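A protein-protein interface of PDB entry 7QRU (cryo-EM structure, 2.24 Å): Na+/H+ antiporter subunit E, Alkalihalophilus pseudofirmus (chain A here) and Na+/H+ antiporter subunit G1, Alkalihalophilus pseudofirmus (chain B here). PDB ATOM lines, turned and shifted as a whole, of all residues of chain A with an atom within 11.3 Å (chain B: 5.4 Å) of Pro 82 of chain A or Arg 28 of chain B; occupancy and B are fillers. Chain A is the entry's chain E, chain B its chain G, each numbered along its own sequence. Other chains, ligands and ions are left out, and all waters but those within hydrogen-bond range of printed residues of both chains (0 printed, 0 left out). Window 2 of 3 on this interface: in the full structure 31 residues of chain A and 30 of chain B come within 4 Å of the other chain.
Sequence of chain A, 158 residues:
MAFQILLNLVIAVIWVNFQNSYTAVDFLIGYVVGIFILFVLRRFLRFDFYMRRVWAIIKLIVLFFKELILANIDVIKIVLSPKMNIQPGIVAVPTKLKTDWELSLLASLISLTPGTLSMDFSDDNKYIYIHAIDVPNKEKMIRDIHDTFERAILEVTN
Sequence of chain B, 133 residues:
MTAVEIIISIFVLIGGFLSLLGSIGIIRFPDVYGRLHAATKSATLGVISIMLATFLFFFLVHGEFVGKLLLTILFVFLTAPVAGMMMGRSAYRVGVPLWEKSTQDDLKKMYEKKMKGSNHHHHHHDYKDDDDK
Of the 15 printed residues of chain A, 7 touch a printed residue of chain B. Hydrophobic or aromatic side chains of chain A that line the printed part of chain B: Ile 78, Val 79, Met 84, Ile 86 and Ile 133. Printed residues of chain B that touch a printed residue of chain A: Ile 24, Gly 25, Arg 28, Phe 29 and Pro 30. Hydrophobic or aromatic side chains of chain B that line the printed part of chain A: Ile 24, Phe 29 and Pro 30. Among the printed residues, 11 pairs touch across the chains.
Among the printed residues, pairs that only touch across the chains: Met 84 of chain A with Arg 28 of chain B (3.4 Å), Val 79 of chain A with Ile 24 of chain B (3.5 Å), Val 79 of chain A with Phe 29 of chain B (3.5 Å), Ile 78 of chain A with Phe 29 of chain B (3.7 Å), Ile 133 of chain A with Phe 29 of chain B (3.8 Å), Ile 86 of chain A with Pro 30 of chain B (3.9 Å), Val 79 of chain A with Gly 25 of chain B (3.9 Å) and Ile 78 of chain A with Arg 28 of chain B (3.9 Å).
OG of Ser 81 of chain A is in hydrogen-bond range of O of Lys 83 of chain A (2.8 Å). OG of Ser 81 of chain A lies within hydrogen-bond range of O of Ile 78 of chain A (2.6 Å).
Of the printed residues of chain B, Ile 78 of chain A touches Arg 28 (3.9 Å) and Phe 29 (3.7 Å). Pro 82 of chain A touches just one residue of chain B: Arg 28. Of the printed residues of chain B, Met 84 of chain A touches Arg 28. Of the printed residues of chain B, Ile 86 of chain A touches Pro 30 (3.9 Å). Gly 25 of chain B touches just one residue of chain A: Val 79. No residue of chain A comes within 4 Å of Ile 27 of chain B. Of chain A, only Ile 86 comes within 4 Å of Pro 30 of chain B. The nearest residue of chain A that does not touch Arg 28 of chain B is Leu 80 of chain A (4.2 Å). The nearest printed residue of chain B that does not touch Ile 86 of chain A is Phe 29 of chain B (4.01 Å).
The backbone carbonyl oxygen of Val 79 of chain A lies within hydrogen-bond range of the guanidinium group of Arg 28 of chain B. O of Pro 82 of chain A lies within hydrogen-bond range of NH2 of Arg 28 of chain B, 3.0 Å away. The backbone carbonyl oxygen of Ser 81 of chain A sits at hydrogen-bond distance from the guanidinium group of Arg 28 of chain B, 2.7 Å away.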
ATOM      1  N   ASP A  74     -10.493  -7.103 -13.622  1.00  0.00           N
ATOM      2  CA  ASP A  74     -11.331  -8.147 -14.160  1.00  0.00           C
ATOM      3  C   ASP A  74     -10.622  -9.492 -14.036  1.00  0.00           C
ATOM      4  O   ASP A  74     -11.277 -10.546 -13.965  1.00  0.00           O
ATOM      5  CB  ASP A  74     -11.769  -7.758 -15.576  1.00  0.00           C
ATOM      6  CG  ASP A  74     -12.253  -8.865 -16.518  1.00  0.00           C
ATOM      7  OD1 ASP A  74     -11.435  -9.719 -16.966  1.00  0.00           O
ATOM      8  OD2 ASP A  74     -13.459  -8.866 -16.817  1.00  0.00           O
ATOM      9  N   VAL A  75      -9.297  -9.482 -14.180  1.00  0.00           N
ATOM     10  CA  VAL A  75      -8.495 -10.689 -14.303  1.00  0.00           C
ATOM     11  C   VAL A  75      -8.298 -11.230 -12.904  1.00  0.00           C
ATOM     12  O   VAL A  75      -8.473 -12.403 -12.663  1.00  0.00           O
ATOM     13  CB  VAL A  75      -7.120 -10.423 -14.939  1.00  0.00           C
ATOM     14  CG1 VAL A  75      -6.152 -11.581 -14.688  1.00  0.00           C
ATOM     15  CG2 VAL A  75      -7.229 -10.157 -16.430  1.00  0.00           C
ATOM     16  N   ILE A  76      -8.006 -10.356 -11.978  1.00  0.00           N
ATOM     17  CA  ILE A  76      -7.932 -10.728 -10.599  1.00  0.00           C
ATOM     18  C   ILE A  76      -9.197 -11.431 -10.111  1.00  0.00           C
ATOM     19  O   ILE A  76      -9.132 -12.479  -9.463  1.00  0.00           O
ATOM     20  CB  ILE A  76      -7.659  -9.508  -9.739  1.00  0.00           C
ATOM     21  CG1 ILE A  76      -6.250  -8.973  -9.947  1.00  0.00           C
ATOM     22  CG2 ILE A  76      -7.836  -9.895  -8.307  1.00  0.00           C
ATOM     23  CD1 ILE A  76      -6.047  -7.667  -9.191  1.00  0.00           C
ATOM     24  N   LYS A  77     -10.339 -10.869 -10.357  1.00  0.00           N
ATOM     25  CA  LYS A  77     -11.572 -11.514  -9.952  1.00  0.00           C
ATOM     26  C   LYS A  77     -11.591 -12.944 -10.466  1.00  0.00           C
ATOM     27  O   LYS A  77     -11.950 -13.829  -9.705  1.00  0.00           O
ATOM     28  CB  LYS A  77     -12.790 -10.734 -10.462  1.00  0.00           C
ATOM     29  CG  LYS A  77     -13.006  -9.407  -9.745  1.00  0.00           C
ATOM     30  CD  LYS A  77     -13.760  -8.389 -10.570  1.00  0.00           C
ATOM     31  CE  LYS A  77     -14.413  -7.267  -9.774  1.00  0.00           C
ATOM     32  NZ  LYS A  77     -13.605  -6.824  -8.610  1.00  0.00           N
ATOM     33  N   ILE A  78     -11.303 -13.155 -11.761  1.00  0.00           N
ATOM     34  CA  ILE A  78     -11.472 -14.444 -12.424  1.00  0.00           C
ATOM     35  C   ILE A  78     -10.488 -15.455 -11.892  1.00  0.00           C
ATOM     36  O   ILE A  78     -10.909 -16.508 -11.494  1.00  0.00           O
ATOM     37  CB  ILE A  78     -11.348 -14.322 -13.960  1.00  0.00           C
ATOM     38  CG1 ILE A  78     -12.560 -13.663 -14.588  1.00  0.00           C
ATOM     39  CG2 ILE A  78     -11.160 -15.663 -14.607  1.00  0.00           C
ATOM     40  CD1 ILE A  78     -12.339 -13.386 -15.994  1.00  0.00           C
ATOM     41  N   VAL A  79      -9.236 -15.065 -11.753  1.00  0.00           N
ATOM     42  CA  VAL A  79      -8.148 -15.951 -11.414  1.00  0.00           C
ATOM     43  C   VAL A  79      -8.185 -16.263  -9.920  1.00  0.00           C
ATOM     44  O   VAL A  79      -7.646 -17.285  -9.533  1.00  0.00           O
ATOM     45  CB  VAL A  79      -6.786 -15.320 -11.816  1.00  0.00           C
ATOM     46  CG1 VAL A  79      -5.552 -15.993 -11.264  1.00  0.00           C
ATOM     47  CG2 VAL A  79      -6.588 -15.307 -13.276  1.00  0.00           C
ATOM     48  N   LEU A  80      -8.656 -15.377  -9.055  1.00  0.00           N
ATOM     49  CA  LEU A  80      -8.699 -15.708  -7.628  1.00  0.00           C
ATOM     50  C   LEU A  80     -10.067 -16.237  -7.209  1.00  0.00           C
ATOM     51  O   LEU A  80     -10.266 -16.475  -6.034  1.00  0.00           O
ATOM     52  CB  LEU A  80      -8.298 -14.511  -6.755  1.00  0.00           C
ATOM     53  CG  LEU A  80      -6.907 -13.980  -7.098  1.00  0.00           C
ATOM     54  CD1 LEU A  80      -6.524 -12.838  -6.236  1.00  0.00           C
ATOM     55  CD2 LEU A  80      -5.879 -15.063  -7.007  1.00  0.00           C
ATOM     56  N   SER A  81     -10.965 -16.469  -8.144  1.00  0.00           N
ATOM     57  CA  SER A  81     -12.236 -17.108  -7.880  1.00  0.00           C
ATOM     58  C   SER A  81     -11.978 -18.600  -7.728  1.00  0.00           C
ATOM     59  O   SER A  81     -11.273 -19.181  -8.554  1.00  0.00           O
ATOM     60  CB  SER A  81     -13.220 -16.857  -8.993  1.00  0.00           C
ATOM     61  OG  SER A  81     -12.841 -17.596 -10.150  1.00  0.00           O
ATOM     62  N   PRO A  82     -12.562 -19.255  -6.693  1.00  0.00           N
ATOM     63  CA  PRO A  82     -12.376 -20.686  -6.474  1.00  0.00           C
ATOM     64  C   PRO A  82     -12.653 -21.475  -7.734  1.00  0.00           C
ATOM     65  O   PRO A  82     -11.902 -22.384  -8.056  1.00  0.00           O
ATOM     66  CB  PRO A  82     -13.435 -20.972  -5.438  1.00  0.00           C
ATOM     67  CG  PRO A  82     -13.414 -19.712  -4.627  1.00  0.00           C
ATOM     68  CD  PRO A  82     -13.469 -18.657  -5.700  1.00  0.00           C
ATOM     69  N   LYS A  83     -13.676 -21.077  -8.491  1.00  0.00           N
ATOM     70  CA  LYS A  83     -13.918 -21.771  -9.741  1.00  0.00           C
ATOM     71  C   LYS A  83     -13.919 -20.792 -10.903  1.00  0.00           C
ATOM     72  O   LYS A  83     -14.578 -19.752 -10.781  1.00  0.00           O
ATOM     73  CB  LYS A  83     -15.267 -22.469  -9.730  1.00  0.00           C
ATOM     74  CG  LYS A  83     -15.522 -23.271 -11.002  1.00  0.00           C
ATOM     75  CD  LYS A  83     -16.989 -23.528 -11.285  1.00  0.00           C
ATOM     76  CE  LYS A  83     -17.760 -24.073 -10.098  1.00  0.00           C
ATOM     77  NZ  LYS A  83     -17.282 -25.418  -9.688  1.00  0.00           N
ATOM     78  N   MET A  84     -13.176 -21.130 -11.984  1.00  0.00           N
ATOM     79  CA  MET A  84     -13.254 -20.365 -13.214  1.00  0.00           C
ATOM     80  C   MET A  84     -14.723 -20.336 -13.593  1.00  0.00           C
ATOM     81  O   MET A  84     -15.275 -21.398 -13.881  1.00  0.00           O
ATOM     82  CB  MET A  84     -12.551 -21.030 -14.406  1.00  0.00           C
ATOM     83  CG  MET A  84     -11.044 -21.009 -14.397  1.00  0.00           C
ATOM     84  SD  MET A  84     -10.278 -19.422 -14.805  1.00  0.00           S
ATOM     85  CE  MET A  84      -9.648 -19.092 -13.162  1.00  0.00           C
ATOM     86  N   ASN A  85     -15.323 -19.146 -13.582  1.00  0.00           N
ATOM     87  CA  ASN A  85     -16.682 -18.962 -14.060  1.00  0.00           C
ATOM     88  C   ASN A  85     -16.584 -18.062 -15.284  1.00  0.00           C
ATOM     89  O   ASN A  85     -16.935 -16.874 -15.203  1.00  0.00           O
ATOM     90  CB  ASN A  85     -17.632 -18.371 -13.003  1.00  0.00           C
ATOM     91  CG  ASN A  85     -17.732 -19.192 -11.735  1.00  0.00           C
ATOM     92  OD1 ASN A  85     -17.895 -20.406 -11.806  1.00  0.00           O
ATOM     93  ND2 ASN A  85     -17.645 -18.547 -10.577  1.00  0.00           N
ATOM     94  N   ILE A  86     -16.106 -18.636 -16.409  1.00  0.00           N
ATOM     95  CA  ILE A  86     -15.997 -17.833 -17.620  1.00  0.00           C
ATOM     96  C   ILE A  86     -16.804 -18.462 -18.745  1.00  0.00           C
ATOM     97  O   ILE A  86     -16.939 -19.680 -18.755  1.00  0.00           O
ATOM     98  CB  ILE A  86     -14.522 -17.614 -18.021  1.00  0.00           C
ATOM     99  CG1 ILE A  86     -13.775 -18.884 -18.284  1.00  0.00           C
ATOM    100  CG2 ILE A  86     -13.753 -16.796 -17.030  1.00  0.00           C
ATOM    101  CD1 ILE A  86     -12.530 -18.574 -19.064  1.00  0.00           C
ATOM    102  N   PRO A  88     -16.323 -17.996 -22.547  1.00  0.00           N
ATOM    103  CA  PRO A  88     -15.569 -17.297 -23.600  1.00  0.00           C
ATOM    104  C   PRO A  88     -16.126 -17.507 -25.017  1.00  0.00           C
ATOM    105  O   PRO A  88     -16.958 -18.368 -25.205  1.00  0.00           O
ATOM    106  CB  PRO A  88     -14.140 -17.842 -23.399  1.00  0.00           C
ATOM    107  CG  PRO A  88     -14.351 -19.160 -22.795  1.00  0.00           C
ATOM    108  CD  PRO A  88     -15.635 -19.152 -22.013  1.00  0.00           C
ATOM    109  N   ILE A 133     -13.876 -13.014 -22.854  1.00  0.00           N
ATOM    110  CA  ILE A 133     -13.839 -13.967 -21.739  1.00  0.00           C
ATOM    111  C   ILE A 133     -15.277 -14.205 -21.260  1.00  0.00           C
ATOM    112  O   ILE A 133     -15.555 -15.265 -20.747  1.00  0.00           O
ATOM    113  CB  ILE A 133     -12.884 -13.469 -20.603  1.00  0.00           C
ATOM    114  CG1 ILE A 133     -12.065 -14.580 -20.035  1.00  0.00           C
ATOM    115  CG2 ILE A 133     -13.623 -12.757 -19.500  1.00  0.00           C
ATOM    116  CD1 ILE A 133     -11.158 -15.178 -21.070  1.00  0.00           C
ATOM    117  N   SER B  23       1.110 -15.069 -14.200  1.00  0.00           N
ATOM    118  CA  SER B  23       1.568 -16.449 -14.202  1.00  0.00           C
ATOM    119  C   SER B  23       0.526 -17.435 -13.662  1.00  0.00           C
ATOM    120  O   SER B  23       0.337 -18.472 -14.288  1.00  0.00           O
ATOM    121  CB  SER B  23       2.874 -16.529 -13.413  1.00  0.00           C
ATOM    122  OG  SER B  23       3.821 -15.692 -14.036  1.00  0.00           O
ATOM    123  N   ILE B  24      -0.125 -17.145 -12.524  1.00  0.00           N
ATOM    124  CA  ILE B  24      -1.192 -17.996 -12.018  1.00  0.00           C
ATOM    125  C   ILE B  24      -2.261 -18.132 -13.121  1.00  0.00           C
ATOM    126  O   ILE B  24      -2.922 -19.145 -13.223  1.00  0.00           O
ATOM    127  CB  ILE B  24      -1.832 -17.443 -10.705  1.00  0.00           C
ATOM    128  CG1 ILE B  24      -0.990 -17.370  -9.416  1.00  0.00           C
ATOM    129  CG2 ILE B  24      -3.068 -18.209 -10.328  1.00  0.00           C
ATOM    130  CD1 ILE B  24       0.075 -18.348  -9.405  1.00  0.00           C
ATOM    131  N   GLY B  25      -2.530 -17.085 -13.891  1.00  0.00           N
ATOM    132  CA  GLY B  25      -3.504 -17.083 -14.965  1.00  0.00           C
ATOM    133  C   GLY B  25      -3.090 -17.987 -16.127  1.00  0.00           C
ATOM    134  O   GLY B  25      -3.943 -18.628 -16.707  1.00  0.00           O
ATOM    135  N   ILE B  26      -1.819 -18.004 -16.486  1.00  0.00           N
ATOM    136  CA  ILE B  26      -1.266 -18.916 -17.479  1.00  0.00           C
ATOM    137  C   ILE B  26      -1.481 -20.376 -17.032  1.00  0.00           C
ATOM    138  O   ILE B  26      -1.416 -21.302 -17.838  1.00  0.00           O
ATOM    139  CB  ILE B  26       0.253 -18.647 -17.656  1.00  0.00           C
ATOM    140  CG1 ILE B  26       0.629 -17.252 -18.150  1.00  0.00           C
ATOM    141  CG2 ILE B  26       0.908 -19.646 -18.557  1.00  0.00           C
ATOM    142  CD1 ILE B  26      -0.069 -16.833 -19.264  1.00  0.00           C
ATOM    143  N   ILE B  27      -1.563 -20.621 -15.745  1.00  0.00           N
ATOM    144  CA  ILE B  27      -1.869 -21.942 -15.217  1.00  0.00           C
ATOM    145  C   ILE B  27      -3.391 -22.146 -15.200  1.00  0.00           C
ATOM    146  O   ILE B  27      -3.857 -23.044 -15.827  1.00  0.00           O
ATOM    147  CB  ILE B  27      -1.293 -22.137 -13.808  1.00  0.00           C
ATOM    148  CG1 ILE B  27       0.223 -22.056 -13.737  1.00  0.00           C
ATOM    149  CG2 ILE B  27      -1.789 -23.428 -13.229  1.00  0.00           C
ATOM    150  CD1 ILE B  27       0.897 -23.081 -14.518  1.00  0.00           C
ATOM    151  N   ARG B  28      -4.183 -21.258 -14.638  1.00  0.00           N
ATOM    152  CA  ARG B  28      -5.593 -21.546 -14.409  1.00  0.00           C
ATOM    153  C   ARG B  28      -6.518 -21.291 -15.625  1.00  0.00           C
ATOM    154  O   ARG B  28      -7.463 -22.013 -15.795  1.00  0.00           O
ATOM    155  CB  ARG B  28      -6.153 -20.715 -13.277  1.00  0.00           C
ATOM    156  CG  ARG B  28      -5.468 -20.960 -11.937  1.00  0.00           C
ATOM    157  CD  ARG B  28      -6.372 -20.407 -10.823  1.00  0.00           C
ATOM    158  NE  ARG B  28      -7.582 -21.215 -10.638  1.00  0.00           N
ATOM    159  CZ  ARG B  28      -8.713 -20.776 -10.132  1.00  0.00           C
ATOM    160  NH1 ARG B  28      -8.895 -19.495  -9.887  1.00  0.00           N
ATOM    161  NH2 ARG B  28      -9.680 -21.626  -9.875  1.00  0.00           N
ATOM    162  N   PHE B  29      -6.270 -20.404 -16.566  1.00  0.00           N
ATOM    163  CA  PHE B  29      -7.208 -20.269 -17.668  1.00  0.00           C
ATOM    164  C   PHE B  29      -7.220 -21.559 -18.475  1.00  0.00           C
ATOM    165  O   PHE B  29      -6.217 -22.242 -18.610  1.00  0.00           O
ATOM    166  CB  PHE B  29      -6.966 -19.035 -18.543  1.00  0.00           C
ATOM    167  CG  PHE B  29      -7.506 -17.749 -17.991  1.00  0.00           C
ATOM    168  CD1 PHE B  29      -8.787 -17.347 -18.333  1.00  0.00           C
ATOM    169  CD2 PHE B  29      -6.697 -16.901 -17.243  1.00  0.00           C
ATOM    170  CE1 PHE B  29      -9.239 -16.100 -17.945  1.00  0.00           C
ATOM    171  CE2 PHE B  29      -7.216 -15.727 -16.730  1.00  0.00           C
ATOM    172  CZ  PHE B  29      -8.466 -15.318 -17.115  1.00  0.00           C
ATOM    173  N   PRO B  30      -8.422 -21.945 -18.982  1.00  0.00           N
ATOM    174  CA  PRO B  30      -8.628 -23.242 -19.624  1.00  0.00           C
ATOM    175  C   PRO B  30      -8.093 -23.457 -21.018  1.00  0.00           C
ATOM    176  O   PRO B  30      -8.093 -24.602 -21.430  1.00  0.00           O
ATOM    177  CB  PRO B  30     -10.101 -23.388 -19.821  1.00  0.00           C
ATOM    178  CG  PRO B  30     -10.608 -21.982 -19.742  1.00  0.00           C
ATOM    179  CD  PRO B  30      -9.686 -21.220 -18.832  1.00  0.00           C
